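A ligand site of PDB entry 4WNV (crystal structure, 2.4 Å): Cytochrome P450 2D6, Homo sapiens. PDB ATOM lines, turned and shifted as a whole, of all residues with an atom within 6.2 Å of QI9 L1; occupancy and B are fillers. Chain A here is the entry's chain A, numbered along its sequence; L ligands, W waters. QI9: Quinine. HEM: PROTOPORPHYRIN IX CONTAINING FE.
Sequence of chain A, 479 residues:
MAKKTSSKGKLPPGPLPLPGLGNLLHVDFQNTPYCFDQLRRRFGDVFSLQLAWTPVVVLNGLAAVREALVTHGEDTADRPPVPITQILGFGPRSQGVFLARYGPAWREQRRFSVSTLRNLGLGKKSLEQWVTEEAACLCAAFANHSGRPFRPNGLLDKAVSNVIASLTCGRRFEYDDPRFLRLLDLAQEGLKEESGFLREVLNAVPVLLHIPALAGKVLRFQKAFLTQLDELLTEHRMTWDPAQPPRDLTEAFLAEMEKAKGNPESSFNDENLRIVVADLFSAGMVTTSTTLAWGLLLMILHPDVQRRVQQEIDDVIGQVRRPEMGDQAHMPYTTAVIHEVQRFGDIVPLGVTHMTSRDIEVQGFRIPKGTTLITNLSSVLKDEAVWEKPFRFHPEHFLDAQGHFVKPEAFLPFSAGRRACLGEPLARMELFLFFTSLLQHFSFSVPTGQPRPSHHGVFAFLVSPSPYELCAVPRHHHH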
ATOM      1  N   PHE A  98     -15.747  -1.940   5.982  1.00  0.00           N
ATOM      2  CA  PHE A  98     -14.628  -2.860   6.197  1.00  0.00           C
ATOM      3  C   PHE A  98     -14.503  -3.923   5.122  1.00  0.00           C
ATOM      4  O   PHE A  98     -13.442  -4.078   4.529  1.00  0.00           O
ATOM      5  CB  PHE A  98     -14.749  -3.545   7.571  1.00  0.00           C
ATOM      6  CG  PHE A  98     -13.407  -3.871   8.212  1.00  0.00           C
ATOM      7  CD1 PHE A  98     -13.021  -3.252   9.381  1.00  0.00           C
ATOM      8  CD2 PHE A  98     -12.544  -4.782   7.647  1.00  0.00           C
ATOM      9  CE1 PHE A  98     -11.805  -3.528   9.965  1.00  0.00           C
ATOM     10  CE2 PHE A  98     -11.324  -5.080   8.251  1.00  0.00           C
ATOM     11  CZ  PHE A  98     -10.961  -4.444   9.415  1.00  0.00           C
ATOM     12  N   LEU A  99     -15.574  -4.666   4.859  1.00  0.00           N
ATOM     13  CA  LEU A  99     -15.531  -5.689   3.826  1.00  0.00           C
ATOM     14  C   LEU A  99     -16.141  -5.240   2.495  1.00  0.00           C
ATOM     15  O   LEU A  99     -16.266  -6.042   1.569  1.00  0.00           O
ATOM     16  CB  LEU A  99     -16.248  -6.961   4.314  1.00  0.00           C
ATOM     17  CG  LEU A  99     -15.540  -7.727   5.440  1.00  0.00           C
ATOM     18  CD1 LEU A  99     -16.258  -9.027   5.746  1.00  0.00           C
ATOM     19  CD2 LEU A  99     -14.077  -8.009   5.089  1.00  0.00           C
ATOM     20  N   LEU A 191     -16.038 -12.683  17.168  1.00  0.00           N
ATOM     21  CA  LEU A 191     -14.681 -12.645  16.649  1.00  0.00           C
ATOM     22  C   LEU A 191     -14.194 -14.088  16.420  1.00  0.00           C
ATOM     23  O   LEU A 191     -13.724 -14.410  15.340  1.00  0.00           O
ATOM     24  CB  LEU A 191     -13.743 -11.876  17.591  1.00  0.00           C
ATOM     25  CG  LEU A 191     -12.306 -11.715  17.103  1.00  0.00           C
ATOM     26  CD1 LEU A 191     -12.298 -11.387  15.610  1.00  0.00           C
ATOM     27  CD2 LEU A 191     -11.542 -10.663  17.894  1.00  0.00           C
ATOM     28  N   GLU A 194     -14.914 -15.824  13.270  1.00  0.00           N
ATOM     29  CA  GLU A 194     -14.142 -15.423  12.096  1.00  0.00           C
ATOM     30  C   GLU A 194     -13.200 -16.566  11.711  1.00  0.00           C
ATOM     31  O   GLU A 194     -12.703 -16.620  10.586  1.00  0.00           O
ATOM     32  CB  GLU A 194     -13.353 -14.154  12.392  1.00  0.00           C
ATOM     33  CG  GLU A 194     -13.265 -13.170  11.264  1.00  0.00           C
ATOM     34  CD  GLU A 194     -14.520 -12.352  11.099  1.00  0.00           C
ATOM     35  OE1 GLU A 194     -14.983 -12.215   9.949  1.00  0.00           O
ATOM     36  OE2 GLU A 194     -15.038 -11.842  12.110  1.00  0.00           O
ATOM     37  N   ARG A 199     -16.766 -21.378   7.572  1.00  0.00           N
ATOM     38  CA  ARG A 199     -16.937 -20.207   6.720  1.00  0.00           C
ATOM     39  C   ARG A 199     -16.182 -20.388   5.400  1.00  0.00           C
ATOM     40  O   ARG A 199     -16.533 -19.787   4.382  1.00  0.00           O
ATOM     41  CB  ARG A 199     -16.481 -18.931   7.426  1.00  0.00           C
ATOM     42  CG  ARG A 199     -15.018 -18.925   7.827  1.00  0.00           C
ATOM     43  CD  ARG A 199     -14.482 -17.502   7.804  1.00  0.00           C
ATOM     44  NE  ARG A 199     -15.371 -16.567   8.500  1.00  0.00           N
ATOM     45  CZ  ARG A 199     -15.837 -15.435   7.972  1.00  0.00           C
ATOM     46  NH1 ARG A 199     -15.498 -15.083   6.737  1.00  0.00           N
ATOM     47  NH2 ARG A 199     -16.633 -14.657   8.701  1.00  0.00           N
ATOM     48  N   GLN A 222     -22.444 -13.016  15.338  1.00  0.00           N
ATOM     49  CA  GLN A 222     -22.422 -11.729  14.658  1.00  0.00           C
ATOM     50  C   GLN A 222     -23.834 -11.267  14.348  1.00  0.00           C
ATOM     51  O   GLN A 222     -24.125 -10.056  14.371  1.00  0.00           O
ATOM     52  CB  GLN A 222     -21.594 -11.780  13.365  1.00  0.00           C
ATOM     53  CG  GLN A 222     -20.109 -11.948  13.574  1.00  0.00           C
ATOM     54  CD  GLN A 222     -19.292 -11.437  12.385  1.00  0.00           C
ATOM     55  OE1 GLN A 222     -19.661 -10.454  11.744  1.00  0.00           O
ATOM     56  NE2 GLN A 222     -18.182 -12.124  12.085  1.00  0.00           N
ATOM     57  N   ALA A 278     -21.801  -1.360  13.075  1.00  0.00           N
ATOM     58  CA  ALA A 278     -21.168  -2.605  13.507  1.00  0.00           C
ATOM     59  C   ALA A 278     -19.710  -2.696  13.071  1.00  0.00           C
ATOM     60  O   ALA A 278     -18.880  -3.209  13.820  1.00  0.00           O
ATOM     61  CB  ALA A 278     -21.931  -3.799  12.965  1.00  0.00           C
ATOM     62  N   ASP A 279     -19.403  -2.199  11.874  1.00  0.00           N
ATOM     63  CA  ASP A 279     -18.030  -2.160  11.393  1.00  0.00           C
ATOM     64  C   ASP A 279     -17.133  -1.318  12.308  1.00  0.00           C
ATOM     65  O   ASP A 279     -16.018  -1.739  12.622  1.00  0.00           O
ATOM     66  CB  ASP A 279     -17.940  -1.609   9.962  1.00  0.00           C
ATOM     67  CG  ASP A 279     -18.190  -2.683   8.902  1.00  0.00           C
ATOM     68  OD1 ASP A 279     -18.292  -2.319   7.705  1.00  0.00           O
ATOM     69  OD2 ASP A 279     -18.277  -3.873   9.256  1.00  0.00           O
ATOM     70  N   SER A 282     -16.638  -3.224  15.603  1.00  0.00           N
ATOM     71  CA  SER A 282     -15.804  -4.410  15.378  1.00  0.00           C
ATOM     72  C   SER A 282     -14.361  -4.024  15.171  1.00  0.00           C
ATOM     73  O   SER A 282     -13.447  -4.648  15.713  1.00  0.00           O
ATOM     74  CB  SER A 282     -16.285  -5.190  14.170  1.00  0.00           C
ATOM     75  OG  SER A 282     -17.439  -5.942  14.482  1.00  0.00           O
ATOM     76  N   ALA A 283     -14.181  -2.974  14.377  1.00  0.00           N
ATOM     77  CA  ALA A 283     -12.849  -2.537  14.002  1.00  0.00           C
ATOM     78  C   ALA A 283     -12.185  -1.759  15.120  1.00  0.00           C
ATOM     79  O   ALA A 283     -10.977  -1.821  15.283  1.00  0.00           O
ATOM     80  CB  ALA A 283     -12.929  -1.675  12.742  1.00  0.00           C
ATOM     81  N   GLY A 284     -12.984  -1.034  15.907  1.00  0.00           N
ATOM     82  CA  GLY A 284     -12.440  -0.145  16.914  1.00  0.00           C
ATOM     83  C   GLY A 284     -12.336  -0.656  18.338  1.00  0.00           C
ATOM     84  O   GLY A 284     -11.635  -0.066  19.162  1.00  0.00           O
ATOM     85  N   VAL A 286     -11.749  -4.296  19.846  1.00  0.00           N
ATOM     86  CA  VAL A 286     -10.755  -5.297  20.180  1.00  0.00           C
ATOM     87  C   VAL A 286      -9.334  -4.824  19.860  1.00  0.00           C
ATOM     88  O   VAL A 286      -8.378  -5.173  20.574  1.00  0.00           O
ATOM     89  CB  VAL A 286     -11.071  -6.631  19.449  1.00  0.00           C
ATOM     90  CG1 VAL A 286     -10.837  -6.487  17.924  1.00  0.00           C
ATOM     91  CG2 VAL A 286     -10.266  -7.792  20.043  1.00  0.00           C
ATOM     92  N   THR A 287      -9.172  -4.003  18.822  1.00  0.00           N
ATOM     93  CA  THR A 287      -7.858  -3.456  18.486  1.00  0.00           C
ATOM     94  C   THR A 287      -7.339  -2.504  19.577  1.00  0.00           C
ATOM     95  O   THR A 287      -6.315  -2.770  20.206  1.00  0.00           O
ATOM     96  CB  THR A 287      -7.889  -2.710  17.144  1.00  0.00           C
ATOM     97  OG1 THR A 287      -8.980  -1.781  17.151  1.00  0.00           O
ATOM     98  CG2 THR A 287      -8.067  -3.690  15.959  1.00  0.00           C
ATOM     99  N   VAL A 348      -2.243  -7.110  14.822  1.00  0.00           N
ATOM    100  CA  VAL A 348      -2.849  -7.588  13.577  1.00  0.00           C
ATOM    101  C   VAL A 348      -1.751  -8.034  12.592  1.00  0.00           C
ATOM    102  O   VAL A 348      -1.542  -7.399  11.538  1.00  0.00           O
ATOM    103  CB  VAL A 348      -3.746  -6.514  12.902  1.00  0.00           C
ATOM    104  CG1 VAL A 348      -4.720  -7.190  11.969  1.00  0.00           C
ATOM    105  CG2 VAL A 348      -4.545  -5.737  13.948  1.00  0.00           C
ATOM    106  N   GLY A 351      -2.657  -8.436   9.027  1.00  0.00           N
ATOM    107  CA  GLY A 351      -3.620  -7.424   8.598  1.00  0.00           C
ATOM    108  C   GLY A 351      -4.985  -7.950   8.169  1.00  0.00           C
ATOM    109  O   GLY A 351      -5.502  -8.898   8.739  1.00  0.00           O
ATOM    110  N   VAL A 352      -5.550  -7.319   7.139  1.00  0.00           N
ATOM    111  CA  VAL A 352      -6.829  -7.757   6.568  1.00  0.00           C
ATOM    112  C   VAL A 352      -6.613  -7.993   5.078  1.00  0.00           C
ATOM    113  O   VAL A 352      -5.926  -7.224   4.416  1.00  0.00           O
ATOM    114  CB  VAL A 352      -7.919  -6.716   6.799  1.00  0.00           C
ATOM    115  CG1 VAL A 352      -9.290  -7.234   6.317  1.00  0.00           C
ATOM    116  CG2 VAL A 352      -7.962  -6.343   8.287  1.00  0.00           C
ATOM    117  N   THR A 353      -7.193  -9.065   4.555  1.00  0.00           N
ATOM    118  CA  THR A 353      -6.874  -9.453   3.176  1.00  0.00           C
ATOM    119  C   THR A 353      -7.363  -8.417   2.153  1.00  0.00           C
ATOM    120  O   THR A 353      -8.396  -7.782   2.346  1.00  0.00           O
ATOM    121  CB  THR A 353      -7.459 -10.824   2.830  1.00  0.00           C
ATOM    122  OG1 THR A 353      -8.848 -10.830   3.161  1.00  0.00           O
ATOM    123  CG2 THR A 353      -6.754 -11.899   3.622  1.00  0.00           C
ATOM    124  N   PHE A 461      -6.064 -14.333  14.596  1.00  0.00           N
ATOM    125  CA  PHE A 461      -6.193 -13.174  13.694  1.00  0.00           C
ATOM    126  C   PHE A 461      -5.637 -11.956  14.383  1.00  0.00           C
ATOM    127  O   PHE A 461      -4.692 -11.339  13.914  1.00  0.00           O
ATOM    128  CB  PHE A 461      -7.647 -12.902  13.253  1.00  0.00           C
ATOM    129  CG  PHE A 461      -8.254 -14.008  12.433  1.00  0.00           C
ATOM    130  CD1 PHE A 461      -9.499 -14.527  12.773  1.00  0.00           C
ATOM    131  CD2 PHE A 461      -7.598 -14.515  11.329  1.00  0.00           C
ATOM    132  CE1 PHE A 461     -10.073 -15.543  12.027  1.00  0.00           C
ATOM    133  CE2 PHE A 461      -8.179 -15.532  10.559  1.00  0.00           C
ATOM    134  CZ  PHE A 461      -9.414 -16.049  10.914  1.00  0.00           C
ATOM    135  N   LEU A 462      -6.266 -11.581  15.502  1.00  0.00           N
ATOM    136  CA  LEU A 462      -5.705 -10.612  16.419  1.00  0.00           C
ATOM    137  C   LEU A 462      -4.766 -11.296  17.406  1.00  0.00           C
ATOM    138  O   LEU A 462      -4.979 -12.447  17.776  1.00  0.00           O
ATOM    139  CB  LEU A 462      -6.826  -9.892  17.174  1.00  0.00           C
ATOM    140  CG  LEU A 462      -7.305  -8.652  16.452  1.00  0.00           C
ATOM    141  CD1 LEU A 462      -8.630  -8.951  15.809  1.00  0.00           C
ATOM    142  CD2 LEU A 462      -7.385  -7.549  17.462  1.00  0.00           C
HETATM  143  O1  QI9 L   1     -13.993  -7.666  14.101  1.00  0.00           O
HETATM  144  C10 QI9 L   1     -13.168  -8.297  13.123  1.00  0.00           C
HETATM  145  C11 QI9 L   1     -13.797  -8.159  11.729  1.00  0.00           C
HETATM  146  N1  QI9 L   1     -15.008  -8.984  11.538  1.00  0.00           N
HETATM  147  C15 QI9 L   1     -16.187  -8.294  12.081  1.00  0.00           C
HETATM  148  C14 QI9 L   1     -16.518  -7.035  11.272  1.00  0.00           C
HETATM  149  C16 QI9 L   1     -15.206  -9.154  10.090  1.00  0.00           C
HETATM  150  C17 QI9 L   1     -15.189  -7.814   9.329  1.00  0.00           C
HETATM  151  C18 QI9 L   1     -13.976  -7.658   8.461  1.00  0.00           C
HETATM  152  C19 QI9 L   1     -12.945  -8.480   8.394  1.00  0.00           C
HETATM  153  C13 QI9 L   1     -15.311  -6.714  10.399  1.00  0.00           C
HETATM  154  C12 QI9 L   1     -14.054  -6.708  11.283  1.00  0.00           C
HETATM  155  C4  QI9 L   1     -11.764  -7.720  13.126  1.00  0.00           C
HETATM  156  C5  QI9 L   1     -11.487  -6.550  13.793  1.00  0.00           C
HETATM  157  C6  QI9 L   1     -10.217  -6.004  13.739  1.00  0.00           C
HETATM  158  N   QI9 L   1      -9.210  -6.520  13.075  1.00  0.00           N
HETATM  159  C7  QI9 L   1      -9.438  -7.695  12.402  1.00  0.00           C
HETATM  160  C3  QI9 L   1     -10.695  -8.344  12.407  1.00  0.00           C
HETATM  161  C2  QI9 L   1     -10.821  -9.585  11.737  1.00  0.00           C
HETATM  162  C8  QI9 L   1      -8.357  -8.296  11.700  1.00  0.00           C
HETATM  163  C9  QI9 L   1      -8.522  -9.495  11.055  1.00  0.00           C
HETATM  164  C1  QI9 L   1      -9.759 -10.141  11.087  1.00  0.00           C
HETATM  165  O   QI9 L   1      -9.849 -11.356  10.454  1.00  0.00           O
HETATM  166  C   QI9 L   1      -8.687 -11.848   9.790  1.00  0.00           C
HETATM  167  CHA HEM L   2      -8.952  -1.158   8.930  1.00  0.00           C
HETATM  168  CHB HEM L   2      -5.640  -1.753  12.452  1.00  0.00           C
HETATM  169  CHC HEM L   2      -8.469   0.981  15.348  1.00  0.00           C
HETATM  170  CHD HEM L   2     -11.834   1.388  11.904  1.00  0.00           C
HETATM  171  C1A HEM L   2      -7.822  -1.594   9.606  1.00  0.00           C
HETATM  172  C2A HEM L   2      -6.758  -2.423   9.074  1.00  0.00           C
HETATM  173  C3A HEM L   2      -5.850  -2.584  10.026  1.00  0.00           C
HETATM  174  C4A HEM L   2      -6.289  -1.850  11.216  1.00  0.00           C
HETATM  175  CMA HEM L   2      -4.595  -3.408   9.863  1.00  0.00           C
HETATM  176  CAA HEM L   2      -6.691  -3.047   7.670  1.00  0.00           C
HETATM  177  CBA HEM L   2      -6.116  -2.114   6.610  1.00  0.00           C
HETATM  178  CGA HEM L   2      -6.041  -2.872   5.300  1.00  0.00           C
HETATM  179  O1A HEM L   2      -7.087  -3.449   4.852  1.00  0.00           O
HETATM  180  O2A HEM L   2      -4.934  -2.901   4.682  1.00  0.00           O
HETATM  181  C1B HEM L   2      -6.089  -1.024  13.564  1.00  0.00           C
HETATM  182  C2B HEM L   2      -5.380  -0.800  14.824  1.00  0.00           C
HETATM  183  C3B HEM L   2      -6.172  -0.045  15.616  1.00  0.00           C
HETATM  184  C4B HEM L   2      -7.397   0.237  14.881  1.00  0.00           C
HETATM  185  CMB HEM L   2      -4.013  -1.343  15.131  1.00  0.00           C
HETATM  186  CAB HEM L   2      -5.970   0.495  17.055  1.00  0.00           C
HETATM  187  CBB HEM L   2      -4.918   0.233  17.841  1.00  0.00           C
HETATM  188  C1C HEM L   2      -9.615   1.362  14.682  1.00  0.00           C
HETATM  189  C2C HEM L   2     -10.637   2.267  15.163  1.00  0.00           C
HETATM  190  C3C HEM L   2     -11.582   2.378  14.214  1.00  0.00           C
HETATM  191  C4C HEM L   2     -11.155   1.551  13.105  1.00  0.00           C
HETATM  192  CMC HEM L   2     -10.606   2.943  16.519  1.00  0.00           C
HETATM  193  CAC HEM L   2     -12.893   3.193  14.168  1.00  0.00           C
HETATM  194  CBC HEM L   2     -13.164   4.280  14.881  1.00  0.00           C
HETATM  195  C1D HEM L   2     -11.372   0.697  10.801  1.00  0.00           C
HETATM  196  C2D HEM L   2     -12.095   0.462   9.567  1.00  0.00           C
HETATM  197  C3D HEM L   2     -11.284  -0.238   8.755  1.00  0.00           C
HETATM  198  C4D HEM L   2     -10.033  -0.468   9.431  1.00  0.00           C
HETATM  199  CMD HEM L   2     -13.518   0.928   9.264  1.00  0.00           C
HETATM  200  CAD HEM L   2     -11.631  -0.698   7.321  1.00  0.00           C
HETATM  201  CBD HEM L   2     -11.089   0.388   6.384  1.00  0.00           C
HETATM  202  CGD HEM L   2     -11.404   0.057   4.943  1.00  0.00           C
HETATM  203  O1D HEM L   2     -11.544   0.987   4.127  1.00  0.00           O
HETATM  204  O2D HEM L   2     -11.548  -1.146   4.611  1.00  0.00           O
HETATM  205  NA  HEM L   2      -7.490  -1.237  10.896  1.00  0.00           N
HETATM  206  NB  HEM L   2      -7.308  -0.385  13.655  1.00  0.00           N
HETATM  207  NC  HEM L   2      -9.969   0.950  13.421  1.00  0.00           N
HETATM  208  ND  HEM L   2     -10.123   0.109  10.684  1.00  0.00           N
HETATM  209 FE   HEM L   2      -8.656  -0.010  12.150  1.00  0.00          FE
HETATM  210  O   HOH W   1      -8.181  -4.223  12.107  1.00  0.00           O
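The side-chain carboxylate (OE2) of Glu 194 is in salt-bridge range of a nitrogen (N1) of QI9 L1, 2.9 Å away.
The backbone carbonyl oxygen (O) of Ser 282 lies close to an oxygen (O1) of QI9 L1.
Phe 98 touches QI9 L1.
CD2 of Leu 99 touches C18 of QI9 L1 (3.4 Å).
Thr 287 touches QI9 L1 (CG2 to C6, 3.9 Å).
Val 348 touches QI9 L1.
O of Gly 351 touches C9 of QI9 L1 (3.9 Å).
Val 352 touches QI9 L1 (CG2 to C8, 3.95 Å).
Phe 461 touches QI9 L1 (CD2 to C, 3.3 Å).
CD1 of Leu 462 touches N of QI9 L1, 3.7 Å away.
Hydrophobic or aromatic side chains within 4 Å of QI9 L1: Phe 98, Leu 99, Val 348, Val 352, Phe 461 and Leu 462.
Within 4 Å of QI9 L1: Phe 98, Leu 99, Glu 194, Ser 282, Thr 287, Val 348, Gly 351, Val 352, Phe 461 and Leu 462.
The nearest printed residue that does not touch QI9 L1 is Leu 191 (4.1 Å).
The side-chain carboxylate of Asp 279 sits at hydrogen-bond distance from the backbone NH of Phe 98 (3.1 Å).
NH2 of Arg 199 is in salt-bridge range of OE1 of Glu 194, at 3.2 Å.
The side-chain carboxylate (OE2) of Glu 194 sits at hydrogen-bond distance from the side-chain amide nitrogen (NE2) of Gln 222.
OG1 of Thr 287 sits at hydrogen-bond distance from O of Ala 283, 2.7 Å away.
OG of Ser 282 is in hydrogen-bond range of O of Ala 278, at 3.2 Å.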
